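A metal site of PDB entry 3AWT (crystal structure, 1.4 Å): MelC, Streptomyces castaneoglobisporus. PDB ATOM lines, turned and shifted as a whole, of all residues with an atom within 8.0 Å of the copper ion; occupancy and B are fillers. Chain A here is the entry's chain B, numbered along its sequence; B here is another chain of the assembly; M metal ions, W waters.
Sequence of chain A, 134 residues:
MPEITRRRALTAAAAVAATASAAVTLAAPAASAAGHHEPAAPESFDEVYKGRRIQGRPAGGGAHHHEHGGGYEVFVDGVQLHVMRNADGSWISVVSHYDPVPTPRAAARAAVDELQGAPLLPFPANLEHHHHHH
The side-chain carboxylate (OE1) of Glu 67 binds the copper ion (1.7 Å).
NE2 of His 82 binds the copper ion, 2.0 Å away.
The copper ion is bound by a ring nitrogen (ND1) of His 68 (2.0 Å).
The backbone carbonyl oxygen (O) of His 68 binds the copper ion (2.1 Å).
The copper ion has four donor atoms within binding distance.
Slightly farther from the copper ion lies the backbone nitrogen (N) of His 68 (2.6 Å).
Slightly farther from the copper ion lies water W1 (2.8 Å).
N of His 68 is in hydrogen-bond range of O of Met 43 of chain B, at 3.0 Å.
The backbone NH (N) of Glu 67 lies close to the side-chain hydroxyl (OG) of Ser 44 of chain B (3.4 Å).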
ATOM      1  N   HIS A  66     -32.637  25.550 -20.453  1.00  0.00           N
ATOM      2  CA  HIS A  66     -32.020  25.130 -21.724  1.00  0.00           C
ATOM      3  C   HIS A  66     -30.570  25.568 -21.841  1.00  0.00           C
ATOM      4  O   HIS A  66     -29.936  25.470 -22.888  1.00  0.00           O
ATOM      5  CB  HIS A  66     -32.866  25.661 -22.891  1.00  0.00           C
ATOM      6  CG  HIS A  66     -33.978  24.722 -23.253  1.00  0.00           C
ATOM      7  ND1 HIS A  66     -35.270  25.112 -23.470  1.00  0.00           N
ATOM      8  CD2 HIS A  66     -33.968  23.376 -23.407  1.00  0.00           C
ATOM      9  CE1 HIS A  66     -36.018  24.060 -23.768  1.00  0.00           C
ATOM     10  NE2 HIS A  66     -35.236  22.991 -23.733  1.00  0.00           N
ATOM     11  N   GLU A  67     -30.008  26.056 -20.748  1.00  0.00           N
ATOM     12  CA  GLU A  67     -28.620  26.493 -20.630  1.00  0.00           C
ATOM     13  C   GLU A  67     -28.205  26.358 -19.180  1.00  0.00           C
ATOM     14  O   GLU A  67     -29.012  25.943 -18.337  1.00  0.00           O
ATOM     15  CB  GLU A  67     -28.464  27.906 -21.176  1.00  0.00           C
ATOM     16  CG  GLU A  67     -29.588  28.857 -20.814  1.00  0.00           C
ATOM     17  CD  GLU A  67     -29.297  29.632 -19.539  1.00  0.00           C
ATOM     18  OE1 GLU A  67     -28.182  29.470 -19.015  1.00  0.00           O
ATOM     19  OE2 GLU A  67     -30.193  30.375 -19.066  1.00  0.00           O
ATOM     20  N   HIS A  68     -26.967  26.671 -18.824  1.00  0.00           N
ATOM     21  CA  HIS A  68     -26.473  26.382 -17.473  1.00  0.00           C
ATOM     22  C   HIS A  68     -26.869  27.456 -16.466  1.00  0.00           C
ATOM     23  O   HIS A  68     -27.331  28.527 -16.869  1.00  0.00           O
ATOM     24  CB  HIS A  68     -24.957  26.285 -17.531  1.00  0.00           C
ATOM     25  CG  HIS A  68     -24.188  27.570 -17.502  1.00  0.00           C
ATOM     26  ND1 HIS A  68     -24.611  28.708 -18.152  1.00  0.00           N
ATOM     27  CD2 HIS A  68     -23.012  27.903 -16.903  1.00  0.00           C
ATOM     28  CE1 HIS A  68     -23.738  29.683 -17.968  1.00  0.00           C
ATOM     29  NE2 HIS A  68     -22.746  29.226 -17.203  1.00  0.00           N
ATOM     30  N   GLY A  69     -26.664  27.204 -15.168  1.00  0.00           N
ATOM     31  CA  GLY A  69     -26.844  28.228 -14.147  1.00  0.00           C
ATOM     32  C   GLY A  69     -25.589  29.063 -13.923  1.00  0.00           C
ATOM     33  O   GLY A  69     -24.723  28.654 -13.131  1.00  0.00           O
ATOM     34  N   GLY A  70     -25.453  30.210 -14.592  1.00  0.00           N
ATOM     35  CA  GLY A  70     -24.251  31.016 -14.597  1.00  0.00           C
ATOM     36  C   GLY A  70     -24.069  31.994 -13.463  1.00  0.00           C
ATOM     37  O   GLY A  70     -25.010  32.663 -13.004  1.00  0.00           O
ATOM     38  N   GLY A  71     -22.823  32.140 -12.975  1.00  0.00           N
ATOM     39  CA  GLY A  71     -22.542  33.112 -11.931  1.00  0.00           C
ATOM     40  C   GLY A  71     -22.285  34.510 -12.460  1.00  0.00           C
ATOM     41  O   GLY A  71     -21.845  35.379 -11.678  1.00  0.00           O
ATOM     42  N   TYR A  72     -22.520  34.713 -13.750  1.00  0.00           N
ATOM     43  CA  TYR A  72     -22.164  36.036 -14.305  1.00  0.00           C
ATOM     44  C   TYR A  72     -23.007  36.323 -15.537  1.00  0.00           C
ATOM     45  O   TYR A  72     -23.269  35.430 -16.341  1.00  0.00           O
ATOM     46  CB  TYR A  72     -20.668  36.082 -14.631  1.00  0.00           C
ATOM     47  CG  TYR A  72     -20.140  37.468 -14.868  1.00  0.00           C
ATOM     48  CD1 TYR A  72     -19.531  38.165 -13.844  1.00  0.00           C
ATOM     49  CD2 TYR A  72     -20.204  38.104 -16.104  1.00  0.00           C
ATOM     50  CE1 TYR A  72     -19.018  39.443 -14.041  1.00  0.00           C
ATOM     51  CE2 TYR A  72     -19.710  39.360 -16.286  1.00  0.00           C
ATOM     52  CZ  TYR A  72     -19.098  40.065 -15.268  1.00  0.00           C
ATOM     53  OH  TYR A  72     -18.631  41.326 -15.491  1.00  0.00           O
ATOM     54  N   GLN A  80     -29.334  39.824 -23.323  1.00  0.00           N
ATOM     55  CA  GLN A  80     -28.412  38.956 -22.617  1.00  0.00           C
ATOM     56  C   GLN A  80     -27.650  38.011 -23.561  1.00  0.00           C
ATOM     57  O   GLN A  80     -28.285  37.350 -24.402  1.00  0.00           O
ATOM     58  CB  GLN A  80     -29.076  38.115 -21.527  1.00  0.00           C
ATOM     59  CG  GLN A  80     -28.091  37.744 -20.425  1.00  0.00           C
ATOM     60  CD  GLN A  80     -28.667  36.909 -19.313  1.00  0.00           C
ATOM     61  OE1 GLN A  80     -27.934  36.067 -18.774  1.00  0.00           O
ATOM     62  NE2 GLN A  80     -29.934  37.163 -19.001  1.00  0.00           N
ATOM     63  N   LEU A  81     -26.352  37.921 -23.370  1.00  0.00           N
ATOM     64  CA  LEU A  81     -25.433  37.070 -24.116  1.00  0.00           C
ATOM     65  C   LEU A  81     -25.104  35.890 -23.215  1.00  0.00           C
ATOM     66  O   LEU A  81     -24.507  36.131 -22.160  1.00  0.00           O
ATOM     67  CB  LEU A  81     -24.145  37.781 -24.496  1.00  0.00           C
ATOM     68  CG  LEU A  81     -23.070  36.927 -25.148  1.00  0.00           C
ATOM     69  CD1 LEU A  81     -23.478  36.511 -26.557  1.00  0.00           C
ATOM     70  CD2 LEU A  81     -21.752  37.683 -25.239  1.00  0.00           C
ATOM     71  N   HIS A  82     -25.460  34.670 -23.587  1.00  0.00           N
ATOM     72  CA  HIS A  82     -25.033  33.574 -22.749  1.00  0.00           C
ATOM     73  C   HIS A  82     -23.517  33.430 -22.764  1.00  0.00           C
ATOM     74  O   HIS A  82     -22.871  33.374 -23.805  1.00  0.00           O
ATOM     75  CB  HIS A  82     -25.684  32.277 -23.266  1.00  0.00           C
ATOM     76  CG  HIS A  82     -25.600  31.209 -22.238  1.00  0.00           C
ATOM     77  ND1 HIS A  82     -24.676  30.206 -22.248  1.00  0.00           N
ATOM     78  CD2 HIS A  82     -26.370  30.989 -21.117  1.00  0.00           C
ATOM     79  CE1 HIS A  82     -24.850  29.416 -21.209  1.00  0.00           C
ATOM     80  NE2 HIS A  82     -25.879  29.864 -20.500  1.00  0.00           N
ATOM     81  N   VAL A  83     -22.896  33.341 -21.603  1.00  0.00           N
ATOM     82  CA  VAL A  83     -21.464  33.188 -21.439  1.00  0.00           C
ATOM     83  C   VAL A  83     -21.235  32.121 -20.367  1.00  0.00           C
ATOM     84  O   VAL A  83     -22.089  31.803 -19.545  1.00  0.00           O
ATOM     85  CB  VAL A  83     -20.771  34.499 -21.049  1.00  0.00           C
ATOM     86  CG1 VAL A  83     -20.975  35.591 -22.095  1.00  0.00           C
ATOM     87  CG2 VAL A  83     -21.296  35.006 -19.691  1.00  0.00           C
ATOM     88  N   MET A  84     -20.018  31.551 -20.411  1.00  0.00           N
ATOM     89  CA  MET A  84     -19.694  30.425 -19.564  1.00  0.00           C
ATOM     90  C   MET A  84     -18.225  30.500 -19.166  1.00  0.00           C
ATOM     91  O   MET A  84     -17.388  30.871 -20.015  1.00  0.00           O
ATOM     92  CB  MET A  84     -19.999  29.108 -20.278  1.00  0.00           C
ATOM     93  CG  MET A  84     -19.288  27.908 -19.691  1.00  0.00           C
ATOM     94  SD  MET A  84     -20.025  26.375 -20.294  1.00  0.00           S
ATOM     95  CE  MET A  84     -21.763  26.776 -20.309  1.00  0.00           C
ATOM     96  N   PHE A 123     -31.598  34.106 -25.672  1.00  0.00           N
ATOM     97  CA  PHE A 123     -31.540  32.666 -25.483  1.00  0.00           C
ATOM     98  C   PHE A 123     -32.758  32.236 -24.669  1.00  0.00           C
ATOM     99  O   PHE A 123     -33.335  33.161 -24.057  1.00  0.00           O
ATOM    100  CB  PHE A 123     -30.290  32.187 -24.746  1.00  0.00           C
ATOM    101  CG  PHE A 123     -30.064  32.795 -23.377  1.00  0.00           C
ATOM    102  CD1 PHE A 123     -30.556  32.201 -22.227  1.00  0.00           C
ATOM    103  CD2 PHE A 123     -29.335  33.962 -23.248  1.00  0.00           C
ATOM    104  CE1 PHE A 123     -30.346  32.778 -20.988  1.00  0.00           C
ATOM    105  CE2 PHE A 123     -29.120  34.539 -22.023  1.00  0.00           C
ATOM    106  CZ  PHE A 123     -29.624  33.952 -20.869  1.00  0.00           C
ATOM    107  N   ILE B  42     -24.612  22.204 -25.586  1.00  0.00           N
ATOM    108  CA  ILE B  42     -23.433  23.051 -25.552  1.00  0.00           C
ATOM    109  C   ILE B  42     -23.605  24.153 -24.531  1.00  0.00           C
ATOM    110  O   ILE B  42     -22.660  24.528 -23.831  1.00  0.00           O
ATOM    111  CB  ILE B  42     -23.203  23.634 -26.970  1.00  0.00           C
ATOM    112  CG1 ILE B  42     -21.791  24.176 -27.211  1.00  0.00           C
ATOM    113  CG2 ILE B  42     -24.192  24.740 -27.315  1.00  0.00           C
ATOM    114  CD1 ILE B  42     -20.870  23.044 -27.650  1.00  0.00           C
ATOM    115  N   MET B  43     -24.823  24.666 -24.390  1.00  0.00           N
ATOM    116  CA  MET B  43     -25.022  25.746 -23.442  1.00  0.00           C
ATOM    117  C   MET B  43     -25.193  25.238 -22.020  1.00  0.00           C
ATOM    118  O   MET B  43     -25.085  26.043 -21.069  1.00  0.00           O
ATOM    119  CB  MET B  43     -26.278  26.565 -23.812  1.00  0.00           C
ATOM    120  CG  MET B  43     -26.119  27.382 -25.077  1.00  0.00           C
ATOM    121  SD  MET B  43     -27.610  28.297 -25.482  1.00  0.00           S
ATOM    122  CE  MET B  43     -27.583  29.655 -24.359  1.00  0.00           C
ATOM    123  N   SER B  44     -25.513  23.957 -21.845  1.00  0.00           N
ATOM    124  CA  SER B  44     -25.786  23.482 -20.485  1.00  0.00           C
ATOM    125  C   SER B  44     -24.613  22.740 -19.862  1.00  0.00           C
ATOM    126  O   SER B  44     -24.412  22.749 -18.628  1.00  0.00           O
ATOM    127  CB  SER B  44     -27.014  22.564 -20.496  1.00  0.00           C
ATOM    128  OG  SER B  44     -28.079  23.239 -21.163  1.00  0.00           O
ATOM    129  N   ASP B  45     -23.815  22.044 -20.678  1.00  0.00           N
ATOM    130  CA  ASP B  45     -22.704  21.290 -20.119  1.00  0.00           C
ATOM    131  C   ASP B  45     -21.709  22.202 -19.416  1.00  0.00           C
ATOM    132  O   ASP B  45     -21.308  23.192 -20.024  1.00  0.00           O
ATOM    133  CB  ASP B  45     -21.915  20.515 -21.172  1.00  0.00           C
ATOM    134  CG  ASP B  45     -22.641  19.387 -21.870  1.00  0.00           C
ATOM    135  OD1 ASP B  45     -22.274  19.138 -23.041  1.00  0.00           O
ATOM    136  OD2 ASP B  45     -23.531  18.748 -21.279  1.00  0.00           O
ATOM    137  N   THR B  46     -21.304  21.929 -18.191  1.00  0.00           N
ATOM    138  CA  THR B  46     -20.394  22.902 -17.557  1.00  0.00           C
ATOM    139  C   THR B  46     -19.309  22.101 -16.836  1.00  0.00           C
ATOM    140  O   THR B  46     -19.505  20.943 -16.428  1.00  0.00           O
ATOM    141  CB  THR B  46     -21.054  23.804 -16.499  1.00  0.00           C
ATOM    142  OG1 THR B  46     -21.777  23.005 -15.551  1.00  0.00           O
ATOM    143  CG2 THR B  46     -22.074  24.755 -17.102  1.00  0.00           C
HETATM  144 CU    CU M   1     -26.503  29.226 -18.703  1.00  0.00          CU
HETATM  145  O   HOH W   1     -26.254  31.913 -18.012  1.00  0.00           O
